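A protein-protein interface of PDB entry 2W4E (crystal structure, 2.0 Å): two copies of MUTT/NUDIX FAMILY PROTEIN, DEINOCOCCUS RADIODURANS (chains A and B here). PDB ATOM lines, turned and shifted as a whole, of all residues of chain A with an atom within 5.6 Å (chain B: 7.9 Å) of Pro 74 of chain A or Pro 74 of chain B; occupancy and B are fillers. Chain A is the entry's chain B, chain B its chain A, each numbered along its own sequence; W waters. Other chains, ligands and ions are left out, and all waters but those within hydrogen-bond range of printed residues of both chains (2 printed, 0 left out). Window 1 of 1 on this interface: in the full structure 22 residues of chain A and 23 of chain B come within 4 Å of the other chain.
The backbone carbonyl oxygen (O) of Tyr 73 of chain B lies within hydrogen-bond range of the backbone NH (N) of Gly 126 of chain A, at 2.8 Å.
OE1 of Gln 75 of chain B lies close to OE1 of Gln 75 of chain A (2.7 Å).
O of Gln 124 of chain B sits at hydrogen-bond distance from N of Tyr 73 of chain A, at 2.8 Å.
The backbone carbonyl oxygen (O) of Tyr 73 of chain A is in hydrogen-bond range of the backbone NH (N) of Gly 126 of chain B, at 2.8 Å.
Pro 74 of chain A touches just these residues of chain B: Pro 74, Gln 75 and Pro 127.
Val 81 of chain A touches none of the printed residues of chain B.
Of the printed residues of chain B, Gly 126 of chain A touches Phe 72 (3.7 Å), Tyr 73 (2.8 Å) and Leu 130 (3.7 Å).
Of chain A, only Pro 74 (3.9 Å) and Pro 127 (3.4 Å) come within 4 Å of Pro 74 of chain B.
Printed residues of chain A within 4 Å of Pro 76 of chain B: Asp 125 (3.1 Å).
Ile 78 of chain B touches none of the printed residues of chain A.
Of the printed residues of chain A, Gly 126 of chain B touches Tyr 73.
Of the printed residues of chain A, Leu 130 of chain B touches Gly 126 (3.7 Å).
The nearest residue of chain B that does not touch Pro 74 of chain A is Gly 126 of chain B (4.8 Å).
CA of Phe 72 of chain A touches O of Gln 124 of chain B, at 3.3 Å.
Tyr 73 of chain A touches Pro 127 of chain B.
CB of Pro 74 of chain A touches O of Pro 74 of chain B (3.9 Å).
Gln 75 of chain B touches Pro 74 of chain A.
O of Pro 74 of chain A touches CD of Pro 127 of chain B, at 3.2 Å.
Gln 75 of chain A touches Phe 83 of chain B (NE2 to CZ, 3.9 Å).
Tyr 73 of chain B touches Asp 125 of chain A.
CG of Pro 76 of chain B touches OD1 of Asp 125 of chain A, 3.1 Å away.
Phe 72 of chain B touches Gly 126 of chain A.
CD of Pro 127 of chain A touches O of Tyr 73 of chain B, 3.7 Å away.
N of Phe 83 of chain B sits at hydrogen-bond distance from O of Phe 72 of chain B, at 2.8 Å.
OD2 of Asp 125 of chain B lies within hydrogen-bond range of OG of Ser 128 of chain B, at 2.6 Å.
O of Phe 72 of chain A sits at hydrogen-bond distance from N of Phe 83 of chain A (2.9 Å).
Pro 74 of chain A touches its own counterpart, Pro 74 of chain B.
Pro 74 of chain A touches Pro 127 of chain B, and with the chains exchanged Pro 127 of chain A touches Pro 74 of chain B.
Gln 75 of chain B touches its own counterpart, Gln 75 of chain A.
Pro 76 of chain A touches Asp 125 of chain B, and with the chains exchanged Asp 125 of chain A touches Pro 76 of chain B.
11 positions are printed for both chains.
Of the 22 printed residues of chain B, 11 touch a printed residue of chain A.
Hydrophobic or aromatic side chains of chain B that line the printed part of chain A: Phe 72, Pro 76, Phe 83, Pro 127 and Leu 130.
Hydrophobic or aromatic side chains of chain A that line the printed part of chain B: Phe 72, Tyr 73, Pro 74, Pro 76 and Pro 127.
Along chain A the printed residues that touch a printed residue of chain B span positions 72 to 127.
Among the printed residues, no Asp or Glu carboxylate lies within 4 Å of a Lys or Arg side-chain nitrogen of the other chain.
Water W1 lies within hydrogen-bond range of the backbone carbonyl oxygen of Pro 74 of chain B and the backbone carbonyl oxygen of Pro 74 of chain A.
Water W2 lies within hydrogen-bond range of OG of Ser 79 of chain B (2.9 Å) and OE1 of Gln 75 of chain A (3.0 Å).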
ATOM      1  N   PHE A  72     -22.617   4.740  13.631  1.00  0.00           N
ATOM      2  CA  PHE A  72     -21.618   4.490  12.623  1.00  0.00           C
ATOM      3  C   PHE A  72     -20.269   4.222  13.287  1.00  0.00           C
ATOM      4  O   PHE A  72     -19.992   4.750  14.382  1.00  0.00           O
ATOM      5  CB  PHE A  72     -21.497   5.673  11.625  1.00  0.00           C
ATOM      6  CG  PHE A  72     -21.136   7.008  12.257  1.00  0.00           C
ATOM      7  CD1 PHE A  72     -19.789   7.384  12.442  1.00  0.00           C
ATOM      8  CD2 PHE A  72     -22.137   7.899  12.650  1.00  0.00           C
ATOM      9  CE1 PHE A  72     -19.449   8.651  13.002  1.00  0.00           C
ATOM     10  CE2 PHE A  72     -21.816   9.152  13.228  1.00  0.00           C
ATOM     11  CZ  PHE A  72     -20.458   9.523  13.400  1.00  0.00           C
ATOM     12  N   TYR A  73     -19.449   3.423  12.613  1.00  0.00           N
ATOM     13  CA  TYR A  73     -18.018   3.226  12.973  1.00  0.00           C
ATOM     14  C   TYR A  73     -17.189   4.352  12.373  1.00  0.00           C
ATOM     15  O   TYR A  73     -17.139   4.470  11.143  1.00  0.00           O
ATOM     16  CB  TYR A  73     -17.503   1.912  12.398  1.00  0.00           C
ATOM     17  CG  TYR A  73     -18.240   0.654  12.898  1.00  0.00           C
ATOM     18  CD1 TYR A  73     -17.916   0.092  14.148  1.00  0.00           C
ATOM     19  CD2 TYR A  73     -19.239   0.026  12.120  1.00  0.00           C
ATOM     20  CE1 TYR A  73     -18.561  -1.076  14.633  1.00  0.00           C
ATOM     21  CE2 TYR A  73     -19.897  -1.167  12.617  1.00  0.00           C
ATOM     22  CZ  TYR A  73     -19.560  -1.684  13.864  1.00  0.00           C
ATOM     23  OH  TYR A  73     -20.155  -2.851  14.353  1.00  0.00           O
ATOM     24  N   PRO A  74     -16.500   5.162  13.224  1.00  0.00           N
ATOM     25  CA  PRO A  74     -15.665   6.222  12.603  1.00  0.00           C
ATOM     26  C   PRO A  74     -14.500   5.643  11.810  1.00  0.00           C
ATOM     27  O   PRO A  74     -14.088   6.208  10.814  1.00  0.00           O
ATOM     28  CB  PRO A  74     -15.128   7.019  13.810  1.00  0.00           C
ATOM     29  CG  PRO A  74     -15.274   6.038  14.987  1.00  0.00           C
ATOM     30  CD  PRO A  74     -16.610   5.387  14.675  1.00  0.00           C
ATOM     31  N   GLN A  75     -13.984   4.521  12.255  1.00  0.00           N
ATOM     32  CA  GLN A  75     -12.815   3.956  11.609  1.00  0.00           C
ATOM     33  C   GLN A  75     -12.713   2.461  11.787  1.00  0.00           C
ATOM     34  O   GLN A  75     -11.794   1.982  12.517  1.00  0.00           O
ATOM     35  CB  GLN A  75     -11.531   4.622  12.150  1.00  0.00           C
ATOM     36  CG  GLN A  75     -10.800   5.407  11.101  1.00  0.00           C
ATOM     37  CD  GLN A  75      -9.422   5.834  11.555  1.00  0.00           C
ATOM     38  OE1 GLN A  75      -9.263   6.469  12.599  1.00  0.00           O
ATOM     39  NE2 GLN A  75      -8.433   5.518  10.755  1.00  0.00           N
ATOM     40  N   PRO A  76     -13.604   1.692  11.109  1.00  0.00           N
ATOM     41  CA  PRO A  76     -13.618   0.233  11.386  1.00  0.00           C
ATOM     42  C   PRO A  76     -12.370  -0.561  10.938  1.00  0.00           C
ATOM     43  O   PRO A  76     -12.210  -1.721  11.352  1.00  0.00           O
ATOM     44  CB  PRO A  76     -14.866  -0.270  10.638  1.00  0.00           C
ATOM     45  CG  PRO A  76     -15.032   0.723   9.518  1.00  0.00           C
ATOM     46  CD  PRO A  76     -14.619   2.065  10.098  1.00  0.00           C
ATOM     47  N   VAL A  81     -14.911   0.926  17.903  1.00  0.00           N
ATOM     48  CA  VAL A  81     -15.724   1.988  18.534  1.00  0.00           C
ATOM     49  C   VAL A  81     -16.887   2.413  17.625  1.00  0.00           C
ATOM     50  O   VAL A  81     -16.731   2.474  16.409  1.00  0.00           O
ATOM     51  CB  VAL A  81     -14.899   3.286  18.970  1.00  0.00           C
ATOM     52  CG1 VAL A  81     -14.477   4.141  17.799  1.00  0.00           C
ATOM     53  CG2 VAL A  81     -15.761   4.231  19.821  1.00  0.00           C
ATOM     54  N   VAL A  82     -18.029   2.723  18.248  1.00  0.00           N
ATOM     55  CA  VAL A  82     -19.221   3.181  17.553  1.00  0.00           C
ATOM     56  C   VAL A  82     -19.591   4.548  18.082  1.00  0.00           C
ATOM     57  O   VAL A  82     -19.665   4.771  19.307  1.00  0.00           O
ATOM     58  CB  VAL A  82     -20.452   2.252  17.777  1.00  0.00           C
ATOM     59  CG1 VAL A  82     -21.628   2.705  16.912  1.00  0.00           C
ATOM     60  CG2 VAL A  82     -20.123   0.831  17.456  1.00  0.00           C
ATOM     61  N   PHE A  83     -19.883   5.441  17.153  1.00  0.00           N
ATOM     62  CA  PHE A  83     -20.407   6.746  17.455  1.00  0.00           C
ATOM     63  C   PHE A  83     -21.937   6.808  17.185  1.00  0.00           C
ATOM     64  O   PHE A  83     -22.397   6.488  16.079  1.00  0.00           O
ATOM     65  CB  PHE A  83     -19.680   7.776  16.579  1.00  0.00           C
ATOM     66  CG  PHE A  83     -18.232   8.032  16.983  1.00  0.00           C
ATOM     67  CD1 PHE A  83     -17.627   7.335  18.031  1.00  0.00           C
ATOM     68  CD2 PHE A  83     -17.458   8.948  16.245  1.00  0.00           C
ATOM     69  CE1 PHE A  83     -16.262   7.607  18.412  1.00  0.00           C
ATOM     70  CE2 PHE A  83     -16.108   9.210  16.606  1.00  0.00           C
ATOM     71  CZ  PHE A  83     -15.519   8.538  17.679  1.00  0.00           C
ATOM     72  N   ASP A 125     -14.196  18.048  11.031  1.00  0.00           N
ATOM     73  CA  ASP A 125     -14.318  16.873  11.860  1.00  0.00           C
ATOM     74  C   ASP A 125     -15.331  15.977  11.139  1.00  0.00           C
ATOM     75  O   ASP A 125     -16.473  16.396  10.939  1.00  0.00           O
ATOM     76  CB  ASP A 125     -14.828  17.344  13.214  1.00  0.00           C
ATOM     77  CG  ASP A 125     -15.225  16.201  14.139  1.00  0.00           C
ATOM     78  OD1 ASP A 125     -14.624  15.110  14.109  1.00  0.00           O
ATOM     79  OD2 ASP A 125     -16.151  16.418  14.930  1.00  0.00           O
ATOM     80  N   GLY A 126     -14.890  14.804  10.673  1.00  0.00           N
ATOM     81  CA  GLY A 126     -15.766  13.864   9.922  1.00  0.00           C
ATOM     82  C   GLY A 126     -17.034  13.434  10.691  1.00  0.00           C
ATOM     83  O   GLY A 126     -18.137  13.491  10.164  1.00  0.00           O
ATOM     84  N   PRO A 127     -16.877  13.008  11.953  1.00  0.00           N
ATOM     85  CA  PRO A 127     -18.056  12.633  12.752  1.00  0.00           C
ATOM     86  C   PRO A 127     -19.095  13.707  12.921  1.00  0.00           C
ATOM     87  O   PRO A 127     -20.293  13.416  12.686  1.00  0.00           O
ATOM     88  CB  PRO A 127     -17.453  12.196  14.088  1.00  0.00           C
ATOM     89  CG  PRO A 127     -16.169  11.569  13.656  1.00  0.00           C
ATOM     90  CD  PRO A 127     -15.636  12.555  12.584  1.00  0.00           C
ATOM     91  N   ALA B   7      -5.061   9.335   3.431  1.00  0.00           N
ATOM     92  CA  ALA B   7      -5.648   8.243   2.656  1.00  0.00           C
ATOM     93  C   ALA B   7      -6.661   8.877   1.718  1.00  0.00           C
ATOM     94  O   ALA B   7      -7.205   9.964   2.009  1.00  0.00           O
ATOM     95  CB  ALA B   7      -6.324   7.242   3.580  1.00  0.00           C
ATOM     96  N   PHE B   9     -10.292   8.277  -0.498  1.00  0.00           N
ATOM     97  CA  PHE B   9     -11.507   7.481  -0.527  1.00  0.00           C
ATOM     98  C   PHE B   9     -12.155   7.820  -1.849  1.00  0.00           C
ATOM     99  O   PHE B   9     -12.218   8.984  -2.236  1.00  0.00           O
ATOM    100  CB  PHE B   9     -12.436   7.847   0.641  1.00  0.00           C
ATOM    101  CG  PHE B   9     -12.102   7.133   1.910  1.00  0.00           C
ATOM    102  CD1 PHE B   9     -12.938   6.132   2.401  1.00  0.00           C
ATOM    103  CD2 PHE B   9     -10.928   7.435   2.606  1.00  0.00           C
ATOM    104  CE1 PHE B   9     -12.608   5.412   3.575  1.00  0.00           C
ATOM    105  CE2 PHE B   9     -10.597   6.721   3.766  1.00  0.00           C
ATOM    106  CZ  PHE B   9     -11.445   5.712   4.244  1.00  0.00           C
ATOM    107  N   GLY B  71     -11.996  17.243   2.006  1.00  0.00           N
ATOM    108  CA  GLY B  71     -11.213  16.447   2.967  1.00  0.00           C
ATOM    109  C   GLY B  71     -11.727  16.515   4.415  1.00  0.00           C
ATOM    110  O   GLY B  71     -12.396  17.487   4.789  1.00  0.00           O
ATOM    111  N   PHE B  72     -11.474  15.481   5.214  1.00  0.00           N
ATOM    112  CA  PHE B  72     -11.936  15.468   6.634  1.00  0.00           C
ATOM    113  C   PHE B  72     -11.014  14.638   7.510  1.00  0.00           C
ATOM    114  O   PHE B  72     -10.346  13.748   7.005  1.00  0.00           O
ATOM    115  CB  PHE B  72     -13.399  14.959   6.802  1.00  0.00           C
ATOM    116  CG  PHE B  72     -13.637  13.527   6.303  1.00  0.00           C
ATOM    117  CD1 PHE B  72     -13.658  12.456   7.207  1.00  0.00           C
ATOM    118  CD2 PHE B  72     -13.911  13.266   4.949  1.00  0.00           C
ATOM    119  CE1 PHE B  72     -13.872  11.124   6.786  1.00  0.00           C
ATOM    120  CE2 PHE B  72     -14.136  11.883   4.501  1.00  0.00           C
ATOM    121  CZ  PHE B  72     -14.146  10.852   5.434  1.00  0.00           C
ATOM    122  N   TYR B  73     -11.020  14.913   8.814  1.00  0.00           N
ATOM    123  CA  TYR B  73     -10.367  14.058   9.814  1.00  0.00           C
ATOM    124  C   TYR B  73     -11.378  13.034  10.352  1.00  0.00           C
ATOM    125  O   TYR B  73     -12.411  13.421  10.910  1.00  0.00           O
ATOM    126  CB  TYR B  73      -9.885  14.890  11.017  1.00  0.00           C
ATOM    127  CG  TYR B  73      -8.974  16.064  10.685  1.00  0.00           C
ATOM    128  CD1 TYR B  73      -7.612  15.877  10.482  1.00  0.00           C
ATOM    129  CD2 TYR B  73      -9.481  17.374  10.627  1.00  0.00           C
ATOM    130  CE1 TYR B  73      -6.758  16.958  10.200  1.00  0.00           C
ATOM    131  CE2 TYR B  73      -8.628  18.469  10.342  1.00  0.00           C
ATOM    132  CZ  TYR B  73      -7.276  18.237  10.123  1.00  0.00           C
ATOM    133  OH  TYR B  73      -6.422  19.293   9.852  1.00  0.00           O
ATOM    134  N   PRO B  74     -11.092  11.742  10.193  1.00  0.00           N
ATOM    135  CA  PRO B  74     -12.038  10.730  10.651  1.00  0.00           C
ATOM    136  C   PRO B  74     -12.113  10.640  12.190  1.00  0.00           C
ATOM    137  O   PRO B  74     -13.148  10.249  12.735  1.00  0.00           O
ATOM    138  CB  PRO B  74     -11.460   9.435  10.051  1.00  0.00           C
ATOM    139  CG  PRO B  74      -9.996   9.693  10.009  1.00  0.00           C
ATOM    140  CD  PRO B  74      -9.929  11.125   9.531  1.00  0.00           C
ATOM    141  N   GLN B  75     -11.030  11.001  12.873  1.00  0.00           N
ATOM    142  CA  GLN B  75     -10.967  10.868  14.325  1.00  0.00           C
ATOM    143  C   GLN B  75      -9.996  11.901  14.914  1.00  0.00           C
ATOM    144  O   GLN B  75      -8.923  11.551  15.383  1.00  0.00           O
ATOM    145  CB  GLN B  75     -10.552   9.449  14.693  1.00  0.00           C
ATOM    146  CG  GLN B  75     -11.732   8.555  15.012  1.00  0.00           C
ATOM    147  CD  GLN B  75     -11.323   7.192  15.555  1.00  0.00           C
ATOM    148  OE1 GLN B  75     -10.629   6.423  14.883  1.00  0.00           O
ATOM    149  NE2 GLN B  75     -11.747   6.895  16.779  1.00  0.00           N
ATOM    150  N   PRO B  76     -10.379  13.189  14.874  1.00  0.00           N
ATOM    151  CA  PRO B  76      -9.411  14.248  15.226  1.00  0.00           C
ATOM    152  C   PRO B  76      -9.058  14.283  16.719  1.00  0.00           C
ATOM    153  O   PRO B  76      -8.120  14.987  17.107  1.00  0.00           O
ATOM    154  CB  PRO B  76     -10.118  15.543  14.792  1.00  0.00           C
ATOM    155  CG  PRO B  76     -11.600  15.220  14.825  1.00  0.00           C
ATOM    156  CD  PRO B  76     -11.700  13.732  14.490  1.00  0.00           C
ATOM    157  N   SER B  77      -9.767  13.507  17.535  1.00  0.00           N
ATOM    158  CA  SER B  77      -9.497  13.470  18.977  1.00  0.00           C
ATOM    159  C   SER B  77      -8.249  12.656  19.228  1.00  0.00           C
ATOM    160  O   SER B  77      -7.446  13.021  20.090  1.00  0.00           O
ATOM    161  CB  SER B  77     -10.704  12.940  19.771  1.00  0.00           C
ATOM    162  OG  SER B  77     -10.935  11.540  19.569  1.00  0.00           O
ATOM    163  N   ILE B  78      -8.061  11.574  18.456  1.00  0.00           N
ATOM    164  CA  ILE B  78      -6.885  10.686  18.629  1.00  0.00           C
ATOM    165  C   ILE B  78      -5.879  10.640  17.480  1.00  0.00           C
ATOM    166  O   ILE B  78      -4.802  10.053  17.624  1.00  0.00           O
ATOM    167  CB  ILE B  78      -7.281   9.250  18.952  1.00  0.00           C
ATOM    168  CG1 ILE B  78      -8.302   8.735  17.934  1.00  0.00           C
ATOM    169  CG2 ILE B  78      -7.800   9.161  20.405  1.00  0.00           C
ATOM    170  CD1 ILE B  78      -8.662   7.247  18.128  1.00  0.00           C
ATOM    171  N   SER B  79      -6.217  11.211  16.331  1.00  0.00           N
ATOM    172  CA  SER B  79      -5.330  11.034  15.182  1.00  0.00           C
ATOM    173  C   SER B  79      -5.285  12.250  14.280  1.00  0.00           C
ATOM    174  O   SER B  79      -6.318  12.883  14.048  1.00  0.00           O
ATOM    175  CB  SER B  79      -5.774   9.787  14.398  1.00  0.00           C
ATOM    176  OG  SER B  79      -5.149   9.730  13.129  1.00  0.00           O
ATOM    177  N   GLY B  80      -4.094  12.567  13.754  1.00  0.00           N
ATOM    178  CA  GLY B  80      -4.001  13.626  12.751  1.00  0.00           C
ATOM    179  C   GLY B  80      -4.233  13.234  11.286  1.00  0.00           C
ATOM    180  O   GLY B  80      -4.078  14.077  10.405  1.00  0.00           O
ATOM    181  N   VAL B  81      -4.621  11.978  11.018  1.00  0.00           N
ATOM    182  CA  VAL B  81      -4.811  11.503   9.624  1.00  0.00           C
ATOM    183  C   VAL B  81      -5.933  12.294   8.937  1.00  0.00           C
ATOM    184  O   VAL B  81      -6.935  12.658   9.591  1.00  0.00           O
ATOM    185  CB  VAL B  81      -5.074   9.985   9.535  1.00  0.00           C
ATOM    186  CG1 VAL B  81      -6.441   9.666  10.049  1.00  0.00           C
ATOM    187  CG2 VAL B  81      -4.988   9.480   8.048  1.00  0.00           C
ATOM    188  N   VAL B  82      -5.723  12.620   7.652  1.00  0.00           N
ATOM    189  CA  VAL B  82      -6.739  13.264   6.821  1.00  0.00           C
ATOM    190  C   VAL B  82      -7.183  12.281   5.729  1.00  0.00           C
ATOM    191  O   VAL B  82      -6.348  11.604   5.094  1.00  0.00           O
ATOM    192  CB  VAL B  82      -6.249  14.588   6.194  1.00  0.00           C
ATOM    193  CG1 VAL B  82      -7.340  15.283   5.380  1.00  0.00           C
ATOM    194  CG2 VAL B  82      -5.746  15.527   7.269  1.00  0.00           C
ATOM    195  N   PHE B  83      -8.500  12.209   5.546  1.00  0.00           N
ATOM    196  CA  PHE B  83      -9.128  11.410   4.500  1.00  0.00           C
ATOM    197  C   PHE B  83      -9.578  12.366   3.416  1.00  0.00           C
ATOM    198  O   PHE B  83     -10.272  13.338   3.701  1.00  0.00           O
ATOM    199  CB  PHE B  83     -10.341  10.655   5.107  1.00  0.00           C
ATOM    200  CG  PHE B  83      -9.956   9.425   5.884  1.00  0.00           C
ATOM    201  CD1 PHE B  83      -8.599   9.111   6.093  1.00  0.00           C
ATOM    202  CD2 PHE B  83     -10.934   8.611   6.462  1.00  0.00           C
ATOM    203  CE1 PHE B  83      -8.231   7.994   6.796  1.00  0.00           C
ATOM    204  CE2 PHE B  83     -10.589   7.473   7.176  1.00  0.00           C
ATOM    205  CZ  PHE B  83      -9.265   7.146   7.366  1.00  0.00           C
ATOM    206  N   TYR B  84      -9.155  12.100   2.177  1.00  0.00           N
ATOM    207  CA  TYR B  84      -9.555  12.881   1.024  1.00  0.00           C
ATOM    208  C   TYR B  84     -10.538  12.129   0.140  1.00  0.00           C
ATOM    209  O   TYR B  84     -10.154  11.167  -0.539  1.00  0.00           O
ATOM    210  CB  TYR B  84      -8.324  13.302   0.191  1.00  0.00           C
ATOM    211  CG  TYR B  84      -7.482  14.313   0.911  1.00  0.00           C
ATOM    212  CD1 TYR B  84      -7.818  15.663   0.897  1.00  0.00           C
ATOM    213  CD2 TYR B  84      -6.348  13.911   1.624  1.00  0.00           C
ATOM    214  CE1 TYR B  84      -7.047  16.602   1.575  1.00  0.00           C
ATOM    215  CE2 TYR B  84      -5.560  14.855   2.308  1.00  0.00           C
ATOM    216  CZ  TYR B  84      -5.930  16.177   2.279  1.00  0.00           C
ATOM    217  OH  TYR B  84      -5.166  17.078   2.964  1.00  0.00           O
ATOM    218  N   GLN B 124     -22.858   1.525   7.850  1.00  0.00           N
ATOM    219  CA  GLN B 124     -22.345   1.885   9.174  1.00  0.00           C
ATOM    220  C   GLN B 124     -20.911   2.397   9.058  1.00  0.00           C
ATOM    221  O   GLN B 124     -20.406   2.925  10.022  1.00  0.00           O
ATOM    222  CB  GLN B 124     -22.368   0.681  10.124  1.00  0.00           C
ATOM    223  CG  GLN B 124     -23.757   0.034  10.387  1.00  0.00           C
ATOM    224  CD  GLN B 124     -23.539  -1.425  10.730  1.00  0.00           C
ATOM    225  OE1 GLN B 124     -23.015  -2.171   9.913  1.00  0.00           O
ATOM    226  NE2 GLN B 124     -23.850  -1.811  11.970  1.00  0.00           N
ATOM    227  N   ASP B 125     -20.252   2.222   7.910  1.00  0.00           N
ATOM    228  CA  ASP B 125     -18.883   2.763   7.741  1.00  0.00           C
ATOM    229  C   ASP B 125     -18.946   4.293   7.669  1.00  0.00           C
ATOM    230  O   ASP B 125     -19.532   4.846   6.734  1.00  0.00           O
ATOM    231  CB  ASP B 125     -18.144   2.196   6.522  1.00  0.00           C
ATOM    232  CG  ASP B 125     -16.701   2.694   6.440  1.00  0.00           C
ATOM    233  OD1 ASP B 125     -15.919   2.420   7.370  1.00  0.00           O
ATOM    234  OD2 ASP B 125     -16.336   3.398   5.490  1.00  0.00           O
ATOM    235  N   GLY B 126     -18.394   4.975   8.672  1.00  0.00           N
ATOM    236  CA  GLY B 126     -18.479   6.454   8.699  1.00  0.00           C
ATOM    237  C   GLY B 126     -17.834   7.172   7.492  1.00  0.00           C
ATOM    238  O   GLY B 126     -18.491   7.994   6.848  1.00  0.00           O
ATOM    239  N   PRO B 127     -16.558   6.889   7.196  1.00  0.00           N
ATOM    240  CA  PRO B 127     -15.892   7.564   6.041  1.00  0.00           C
ATOM    241  C   PRO B 127     -16.630   7.337   4.701  1.00  0.00           C
ATOM    242  O   PRO B 127     -16.764   8.280   3.891  1.00  0.00           O
ATOM    243  CB  PRO B 127     -14.502   6.931   6.005  1.00  0.00           C
ATOM    244  CG  PRO B 127     -14.220   6.505   7.457  1.00  0.00           C
ATOM    245  CD  PRO B 127     -15.604   6.071   7.984  1.00  0.00           C
ATOM    246  N   SER B 128     -17.122   6.124   4.481  1.00  0.00           N
ATOM    247  CA  SER B 128     -17.935   5.845   3.290  1.00  0.00           C
ATOM    248  C   SER B 128     -19.226   6.584   3.315  1.00  0.00           C
ATOM    249  O   SER B 128     -19.620   7.122   2.283  1.00  0.00           O
ATOM    250  CB  SER B 128     -18.209   4.337   3.066  1.00  0.00           C
ATOM    251  OG  SER B 128     -16.978   3.627   2.946  1.00  0.00           O
ATOM    252  N   LEU B 130     -19.928   9.398   4.850  1.00  0.00           N
ATOM    253  CA  LEU B 130     -19.752  10.851   4.717  1.00  0.00           C
ATOM    254  C   LEU B 130     -19.466  11.160   3.236  1.00  0.00           C
ATOM    255  O   LEU B 130     -19.931  12.143   2.711  1.00  0.00           O
ATOM    256  CB  LEU B 130     -18.595  11.365   5.599  1.00  0.00           C
ATOM    257  CG  LEU B 130     -18.226  12.851   5.493  1.00  0.00           C
ATOM    258  CD1 LEU B 130     -19.480  13.819   5.577  1.00  0.00           C
ATOM    259  CD2 LEU B 130     -17.221  13.204   6.563  1.00  0.00           C
HETATM  260  O   HOH W   1     -14.919   9.044  11.059  1.00  0.00           O
HETATM  261  O   HOH W   2      -6.388   7.144  12.459  1.00  0.00           O
